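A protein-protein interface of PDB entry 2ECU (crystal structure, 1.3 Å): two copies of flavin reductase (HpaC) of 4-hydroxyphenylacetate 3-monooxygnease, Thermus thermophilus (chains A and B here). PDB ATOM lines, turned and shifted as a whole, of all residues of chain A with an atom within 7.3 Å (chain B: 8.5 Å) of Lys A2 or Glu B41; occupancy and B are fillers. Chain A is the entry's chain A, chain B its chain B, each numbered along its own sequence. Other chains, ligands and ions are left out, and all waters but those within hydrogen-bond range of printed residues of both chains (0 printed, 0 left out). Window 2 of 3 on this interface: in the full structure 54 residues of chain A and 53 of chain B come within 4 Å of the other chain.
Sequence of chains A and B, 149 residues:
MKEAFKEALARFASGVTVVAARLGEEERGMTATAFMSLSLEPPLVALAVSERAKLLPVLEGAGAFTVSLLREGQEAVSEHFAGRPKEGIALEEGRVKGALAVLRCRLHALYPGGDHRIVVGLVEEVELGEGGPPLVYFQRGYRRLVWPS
Met A1 touches none of the printed residues of chain B.
Printed residues of chain B within 4 Å of Lys A2: Leu B40 (3.0 Å) and Glu B41 (3.1 Å).
No residue of chain B comes within 4 Å of Glu A3.
Of the printed residues of chain B, Asp A115 touches Leu B38, Ser B39, Leu B40 and Glu B41.
Glu B41 touches just these residues of chain A: Lys A2 (3.1 Å) and Asp A115 (2.9 Å).
Of the printed residues of chain A, Leu B44 touches Phe A5, Gly A113 and Gly A114.
His B108 touches none of the printed residues of chain A.
No position is printed for both chains.
Of the 21 pairs that touch across the chains among the printed residues, none has its exchanged pair printed and touching as well.
The side-chain hydroxyl (OG) of Ser B39 is in hydrogen-bond range of the backbone carbonyl oxygen (O) of Pro B42.
N of Val B123 is in hydrogen-bond range of O of Pro B43.
OG of Ser B39 lies within hydrogen-bond range of N of Glu B41, 3.5 Å away.
The backbone NH of Leu B44 is in hydrogen-bond range of the backbone carbonyl oxygen of Ser B39 (3.0 Å).
The side-chain carboxylate (OD1) of Asp A115 sits at hydrogen-bond distance from a ring nitrogen (ND1) of His A116, at 2.6 Å.
The backbone carbonyl oxygen of Met A1 is in hydrogen-bond range of the side-chain amino group of Lys A6.
Lys A2 touches Leu B40.
O of Ala A4 touches CG1 of Val B126, 3.7 Å away.
CE2 of Phe A5 touches CB of Pro B43, at 3.7 Å.
Phe A5 touches Val B123 (CE1 to CG2, 3.5 Å).
CG of Leu B38 touches O of Gly A113 (3.5 Å).
Leu B44 touches Gly A113 (CD1 to C, 3.8 Å).
Ser B39 touches Gly A114.
Gly A114 touches Pro B42.
N of Gly A114 touches CD1 of Leu B44, 3.7 Å away.
Asp A115 touches Leu B38.
The side-chain carboxylate of Asp A115 lies within hydrogen-bond range of the backbone NH of Glu B41, 2.9 Å away.
The side-chain amino group of Lys A2 lies within salt-bridge range of the side-chain carboxylate of Glu B41, at 3.1 Å.
The side-chain carboxylate (OD2) of Asp A115 lies within hydrogen-bond range of the backbone NH (N) of Leu B40 (3.0 Å).
The backbone carbonyl oxygen (O) of Leu B38 lies close to a ring nitrogen (ND1) of His A116 (3.2 Å).
The side-chain hydroxyl (OG) of Ser B39 lies within hydrogen-bond range of the backbone NH (N) of Asp A115 (2.9 Å).
Of the 11 printed residues of chain B, 9 touch a printed residue of chain A.
Hydrophobic or aromatic side chains of chain B that line the printed part of chain A: Leu B38, Leu B40, Pro B42, Pro B43, Leu B44, Val B123 and Val B126.
Along chain B the printed residues that touch a printed residue of chain A span positions 38 to 126.
Of the 12 printed residues of chain A, 9 touch a printed residue of chain B.
Hydrophobic or aromatic side chains of chain A within 4 Å of the printed part of chain B: Ala A4, Phe A5, Ala A8 and His A116.
Along chain A the printed residues that touch a printed residue of chain B span positions 2 to 116.
Among the printed residues, 21 pairs touch across the chains.
Among the printed residues, Asp or Glu carboxylates within 4 Å of a Lys or Arg side-chain nitrogen of the other chain: Lys A2 with Glu B41 (3.1 Å).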
ATOM      1  N   MET A   1     -25.419 -27.154 -27.255  1.00  0.00           N
ATOM      2  CA  MET A   1     -26.625 -26.281 -27.137  1.00  0.00           C
ATOM      3  C   MET A   1     -26.649 -25.199 -28.216  1.00  0.00           C
ATOM      4  O   MET A   1     -25.617 -24.887 -28.813  1.00  0.00           O
ATOM      5  CB  MET A   1     -26.658 -25.616 -25.760  1.00  0.00           C
ATOM      6  CG  MET A   1     -26.614 -26.597 -24.604  1.00  0.00           C
ATOM      7  SD  MET A   1     -27.941 -27.815 -24.686  1.00  0.00           S
ATOM      8  CE  MET A   1     -27.671 -28.713 -23.166  1.00  0.00           C
ATOM      9  N   LYS A   2     -27.837 -24.645 -28.456  1.00  0.00           N
ATOM     10  CA  LYS A   2     -28.039 -23.578 -29.438  1.00  0.00           C
ATOM     11  C   LYS A   2     -27.352 -23.853 -30.773  1.00  0.00           C
ATOM     12  O   LYS A   2     -26.774 -22.954 -31.387  1.00  0.00           O
ATOM     13  CB  LYS A   2     -27.550 -22.249 -28.856  1.00  0.00           C
ATOM     14  CG  LYS A   2     -28.231 -21.890 -27.542  1.00  0.00           C
ATOM     15  CD  LYS A   2     -27.842 -20.511 -27.052  1.00  0.00           C
ATOM     16  CE  LYS A   2     -28.595 -20.154 -25.779  1.00  0.00           C
ATOM     17  NZ  LYS A   2     -28.302 -21.105 -24.672  1.00  0.00           N
ATOM     18  N   GLU A   3     -27.440 -25.100 -31.226  1.00  0.00           N
ATOM     19  CA  GLU A   3     -26.815 -25.509 -32.477  1.00  0.00           C
ATOM     20  C   GLU A   3     -27.209 -24.678 -33.698  1.00  0.00           C
ATOM     21  O   GLU A   3     -26.343 -24.254 -34.453  1.00  0.00           O
ATOM     22  CB  GLU A   3     -27.108 -26.986 -32.756  1.00  0.00           C
ATOM     23  CG  GLU A   3     -26.242 -27.983 -31.993  1.00  0.00           C
ATOM     24  CD  GLU A   3     -26.360 -27.860 -30.487  1.00  0.00           C
ATOM     25  OE1 GLU A   3     -27.489 -27.679 -29.988  1.00  0.00           O
ATOM     26  OE2 GLU A   3     -25.319 -27.959 -29.800  1.00  0.00           O
ATOM     27  N   ALA A   4     -28.504 -24.447 -33.903  1.00  0.00           N
ATOM     28  CA  ALA A   4     -28.941 -23.675 -35.069  1.00  0.00           C
ATOM     29  C   ALA A   4     -28.411 -22.242 -35.052  1.00  0.00           C
ATOM     30  O   ALA A   4     -27.955 -21.730 -36.077  1.00  0.00           O
ATOM     31  CB  ALA A   4     -30.462 -23.673 -35.161  1.00  0.00           C
ATOM     32  N   PHE A   5     -28.486 -21.600 -33.890  1.00  0.00           N
ATOM     33  CA  PHE A   5     -28.002 -20.230 -33.724  1.00  0.00           C
ATOM     34  C   PHE A   5     -26.509 -20.166 -34.046  1.00  0.00           C
ATOM     35  O   PHE A   5     -26.059 -19.280 -34.771  1.00  0.00           O
ATOM     36  CB  PHE A   5     -28.274 -19.775 -32.286  1.00  0.00           C
ATOM     37  CG  PHE A   5     -27.686 -18.436 -31.933  1.00  0.00           C
ATOM     38  CD1 PHE A   5     -28.005 -17.293 -32.662  1.00  0.00           C
ATOM     39  CD2 PHE A   5     -26.841 -18.314 -30.836  1.00  0.00           C
ATOM     40  CE1 PHE A   5     -27.490 -16.046 -32.294  1.00  0.00           C
ATOM     41  CE2 PHE A   5     -26.323 -17.077 -30.464  1.00  0.00           C
ATOM     42  CZ  PHE A   5     -26.648 -15.942 -31.193  1.00  0.00           C
ATOM     43  N   LYS A   6     -25.747 -21.118 -33.517  1.00  0.00           N
ATOM     44  CA  LYS A   6     -24.313 -21.161 -33.775  1.00  0.00           C
ATOM     45  C   LYS A   6     -24.022 -21.388 -35.255  1.00  0.00           C
ATOM     46  O   LYS A   6     -23.086 -20.809 -35.802  1.00  0.00           O
ATOM     47  CB  LYS A   6     -23.657 -22.266 -32.950  1.00  0.00           C
ATOM     48  CG  LYS A   6     -23.601 -21.975 -31.469  1.00  0.00           C
ATOM     49  CD  LYS A   6     -23.030 -23.169 -30.736  1.00  0.00           C
ATOM     50  CE  LYS A   6     -22.976 -22.937 -29.241  1.00  0.00           C
ATOM     51  NZ  LYS A   6     -22.538 -24.180 -28.541  1.00  0.00           N
ATOM     52  N   GLU A   7     -24.826 -22.225 -35.904  1.00  0.00           N
ATOM     53  CA  GLU A   7     -24.631 -22.505 -37.322  1.00  0.00           C
ATOM     54  C   GLU A   7     -24.903 -21.243 -38.133  1.00  0.00           C
ATOM     55  O   GLU A   7     -24.172 -20.930 -39.070  1.00  0.00           O
ATOM     56  CB  GLU A   7     -25.564 -23.639 -37.765  1.00  0.00           C
ATOM     57  CG  GLU A   7     -25.501 -23.995 -39.250  1.00  0.00           C
ATOM     58  CD  GLU A   7     -24.109 -24.383 -39.722  1.00  0.00           C
ATOM     59  OE1 GLU A   7     -23.386 -25.065 -38.965  1.00  0.00           O
ATOM     60  OE2 GLU A   7     -23.744 -24.021 -40.864  1.00  0.00           O
ATOM     61  N   ALA A   8     -25.950 -20.514 -37.767  1.00  0.00           N
ATOM     62  CA  ALA A   8     -26.280 -19.281 -38.477  1.00  0.00           C
ATOM     63  C   ALA A   8     -25.128 -18.281 -38.379  1.00  0.00           C
ATOM     64  O   ALA A   8     -24.762 -17.648 -39.367  1.00  0.00           O
ATOM     65  CB  ALA A   8     -27.554 -18.676 -37.909  1.00  0.00           C
ATOM     66  N   GLY A 113     -24.442  -6.686 -22.925  1.00  0.00           N
ATOM     67  CA  GLY A 113     -24.496  -7.520 -24.114  1.00  0.00           C
ATOM     68  C   GLY A 113     -24.621  -8.998 -23.794  1.00  0.00           C
ATOM     69  O   GLY A 113     -24.008  -9.834 -24.453  1.00  0.00           O
ATOM     70  N   GLY A 114     -25.429  -9.328 -22.790  1.00  0.00           N
ATOM     71  CA  GLY A 114     -25.592 -10.718 -22.411  1.00  0.00           C
ATOM     72  C   GLY A 114     -24.328 -11.216 -21.740  1.00  0.00           C
ATOM     73  O   GLY A 114     -23.894 -10.638 -20.741  1.00  0.00           O
ATOM     74  N   ASP A 115     -23.728 -12.277 -22.272  1.00  0.00           N
ATOM     75  CA  ASP A 115     -22.497 -12.785 -21.684  1.00  0.00           C
ATOM     76  C   ASP A 115     -21.271 -12.036 -22.211  1.00  0.00           C
ATOM     77  O   ASP A 115     -20.133 -12.396 -21.916  1.00  0.00           O
ATOM     78  CB  ASP A 115     -22.348 -14.303 -21.899  1.00  0.00           C
ATOM     79  CG  ASP A 115     -22.471 -14.724 -23.351  1.00  0.00           C
ATOM     80  OD1 ASP A 115     -22.052 -13.961 -24.246  1.00  0.00           O
ATOM     81  OD2 ASP A 115     -22.969 -15.845 -23.594  1.00  0.00           O
ATOM     82  N   HIS A 116     -21.524 -10.987 -22.991  1.00  0.00           N
ATOM     83  CA  HIS A 116     -20.469 -10.130 -23.531  1.00  0.00           C
ATOM     84  C   HIS A 116     -20.825  -8.686 -23.216  1.00  0.00           C
ATOM     85  O   HIS A 116     -21.961  -8.379 -22.861  1.00  0.00           O
ATOM     86  CB  HIS A 116     -20.349 -10.265 -25.052  1.00  0.00           C
ATOM     87  CG  HIS A 116     -19.571 -11.459 -25.498  1.00  0.00           C
ATOM     88  ND1 HIS A 116     -19.964 -12.751 -25.224  1.00  0.00           N
ATOM     89  CD2 HIS A 116     -18.413 -11.558 -26.194  1.00  0.00           C
ATOM     90  CE1 HIS A 116     -19.082 -13.593 -25.731  1.00  0.00           C
ATOM     91  NE2 HIS A 116     -18.130 -12.895 -26.324  1.00  0.00           N
ATOM     92  N   LEU B  38     -23.258 -11.385 -30.602  1.00  0.00           N
ATOM     93  CA  LEU B  38     -23.010 -10.676 -29.357  1.00  0.00           C
ATOM     94  C   LEU B  38     -22.963 -11.560 -28.121  1.00  0.00           C
ATOM     95  O   LEU B  38     -22.044 -11.442 -27.310  1.00  0.00           O
ATOM     96  CB  LEU B  38     -24.067  -9.584 -29.163  1.00  0.00           C
ATOM     97  CG  LEU B  38     -24.037  -8.808 -27.843  1.00  0.00           C
ATOM     98  CD1 LEU B  38     -22.685  -8.127 -27.672  1.00  0.00           C
ATOM     99  CD2 LEU B  38     -25.162  -7.788 -27.830  1.00  0.00           C
ATOM    100  N   SER B  39     -23.935 -12.455 -27.987  1.00  0.00           N
ATOM    101  CA  SER B  39     -24.005 -13.310 -26.810  1.00  0.00           C
ATOM    102  C   SER B  39     -24.541 -14.700 -27.123  1.00  0.00           C
ATOM    103  O   SER B  39     -25.309 -14.883 -28.068  1.00  0.00           O
ATOM    104  CB  SER B  39     -24.904 -12.633 -25.767  1.00  0.00           C
ATOM    105  OG  SER B  39     -25.057 -13.417 -24.593  1.00  0.00           O
ATOM    106  N   LEU B  40     -24.122 -15.677 -26.321  1.00  0.00           N
ATOM    107  CA  LEU B  40     -24.579 -17.052 -26.477  1.00  0.00           C
ATOM    108  C   LEU B  40     -25.776 -17.248 -25.547  1.00  0.00           C
ATOM    109  O   LEU B  40     -26.808 -17.781 -25.949  1.00  0.00           O
ATOM    110  CB  LEU B  40     -23.456 -18.027 -26.118  1.00  0.00           C
ATOM    111  CG  LEU B  40     -23.717 -19.513 -26.375  1.00  0.00           C
ATOM    112  CD1 LEU B  40     -24.042 -19.734 -27.847  1.00  0.00           C
ATOM    113  CD2 LEU B  40     -22.489 -20.317 -25.974  1.00  0.00           C
ATOM    114  N   GLU B  41     -25.635 -16.806 -24.301  1.00  0.00           N
ATOM    115  CA  GLU B  41     -26.717 -16.906 -23.328  1.00  0.00           C
ATOM    116  C   GLU B  41     -26.910 -15.577 -22.609  1.00  0.00           C
ATOM    117  O   GLU B  41     -26.095 -15.189 -21.768  1.00  0.00           O
ATOM    118  CB  GLU B  41     -26.439 -18.009 -22.302  1.00  0.00           C
ATOM    119  CG  GLU B  41     -27.502 -18.107 -21.210  1.00  0.00           C
ATOM    120  CD  GLU B  41     -28.902 -18.354 -21.758  1.00  0.00           C
ATOM    121  OE1 GLU B  41     -29.871 -18.277 -20.972  1.00  0.00           O
ATOM    122  OE2 GLU B  41     -29.038 -18.632 -22.968  1.00  0.00           O
ATOM    123  N   PRO B  42     -27.981 -14.845 -22.953  1.00  0.00           N
ATOM    124  CA  PRO B  42     -28.974 -15.220 -23.963  1.00  0.00           C
ATOM    125  C   PRO B  42     -28.394 -15.110 -25.373  1.00  0.00           C
ATOM    126  O   PRO B  42     -27.332 -14.516 -25.568  1.00  0.00           O
ATOM    127  CB  PRO B  42     -30.094 -14.216 -23.722  1.00  0.00           C
ATOM    128  CG  PRO B  42     -29.343 -12.993 -23.314  1.00  0.00           C
ATOM    129  CD  PRO B  42     -28.317 -13.543 -22.349  1.00  0.00           C
ATOM    130  N   PRO B  43     -29.080 -15.694 -26.372  1.00  0.00           N
ATOM    131  CA  PRO B  43     -28.604 -15.641 -27.757  1.00  0.00           C
ATOM    132  C   PRO B  43     -28.893 -14.262 -28.348  1.00  0.00           C
ATOM    133  O   PRO B  43     -30.029 -13.963 -28.711  1.00  0.00           O
ATOM    134  CB  PRO B  43     -29.398 -16.758 -28.430  1.00  0.00           C
ATOM    135  CG  PRO B  43     -30.704 -16.731 -27.687  1.00  0.00           C
ATOM    136  CD  PRO B  43     -30.278 -16.547 -26.248  1.00  0.00           C
ATOM    137  N   LEU B  44     -27.861 -13.427 -28.441  1.00  0.00           N
ATOM    138  CA  LEU B  44     -28.022 -12.065 -28.949  1.00  0.00           C
ATOM    139  C   LEU B  44     -27.109 -11.716 -30.110  1.00  0.00           C
ATOM    140  O   LEU B  44     -26.000 -12.245 -30.233  1.00  0.00           O
ATOM    141  CB  LEU B  44     -27.738 -11.048 -27.836  1.00  0.00           C
ATOM    142  CG  LEU B  44     -28.391 -11.197 -26.462  1.00  0.00           C
ATOM    143  CD1 LEU B  44     -27.828 -10.142 -25.513  1.00  0.00           C
ATOM    144  CD2 LEU B  44     -29.900 -11.055 -26.591  1.00  0.00           C
ATOM    145  N   HIS B 108     -34.357  -6.636 -28.211  1.00  0.00           N
ATOM    146  CA  HIS B 108     -33.882  -6.785 -26.838  1.00  0.00           C
ATOM    147  C   HIS B 108     -33.511  -5.468 -26.160  1.00  0.00           C
ATOM    148  O   HIS B 108     -33.896  -5.219 -25.014  1.00  0.00           O
ATOM    149  CB  HIS B 108     -32.673  -7.723 -26.843  1.00  0.00           C
ATOM    150  CG  HIS B 108     -32.210  -8.139 -25.482  1.00  0.00           C
ATOM    151  ND1 HIS B 108     -32.956  -8.952 -24.656  1.00  0.00           N
ATOM    152  CD2 HIS B 108     -31.061  -7.877 -24.816  1.00  0.00           C
ATOM    153  CE1 HIS B 108     -32.283  -9.177 -23.542  1.00  0.00           C
ATOM    154  NE2 HIS B 108     -31.130  -8.536 -23.613  1.00  0.00           N
ATOM    155  N   LEU B 122     -32.705 -10.455 -29.679  1.00  0.00           N
ATOM    156  CA  LEU B 122     -32.692 -11.733 -28.979  1.00  0.00           C
ATOM    157  C   LEU B 122     -33.247 -12.721 -30.003  1.00  0.00           C
ATOM    158  O   LEU B 122     -34.401 -12.613 -30.416  1.00  0.00           O
ATOM    159  CB  LEU B 122     -33.600 -11.676 -27.748  1.00  0.00           C
ATOM    160  CG  LEU B 122     -33.882 -12.996 -27.026  1.00  0.00           C
ATOM    161  CD1 LEU B 122     -32.604 -13.524 -26.410  1.00  0.00           C
ATOM    162  CD2 LEU B 122     -34.943 -12.778 -25.954  1.00  0.00           C
ATOM    163  N   VAL B 123     -32.424 -13.677 -30.418  1.00  0.00           N
ATOM    164  CA  VAL B 123     -32.844 -14.650 -31.418  1.00  0.00           C
ATOM    165  C   VAL B 123     -33.884 -15.630 -30.886  1.00  0.00           C
ATOM    166  O   VAL B 123     -33.629 -16.367 -29.932  1.00  0.00           O
ATOM    167  CB  VAL B 123     -31.630 -15.435 -31.961  1.00  0.00           C
ATOM    168  CG1 VAL B 123     -32.071 -16.409 -33.049  1.00  0.00           C
ATOM    169  CG2 VAL B 123     -30.597 -14.463 -32.512  1.00  0.00           C
ATOM    170  N   VAL B 126     -34.537 -19.498 -35.899  1.00  0.00           N
ATOM    171  CA  VAL B 126     -33.451 -19.568 -36.866  1.00  0.00           C
ATOM    172  C   VAL B 126     -33.897 -20.388 -38.070  1.00  0.00           C
ATOM    173  O   VAL B 126     -34.460 -21.475 -37.920  1.00  0.00           O
ATOM    174  CB  VAL B 126     -32.185 -20.245 -36.286  1.00  0.00           C
ATOM    175  CG1 VAL B 126     -31.125 -20.373 -37.374  1.00  0.00           C
ATOM    176  CG2 VAL B 126     -31.642 -19.442 -35.118  1.00  0.00           C
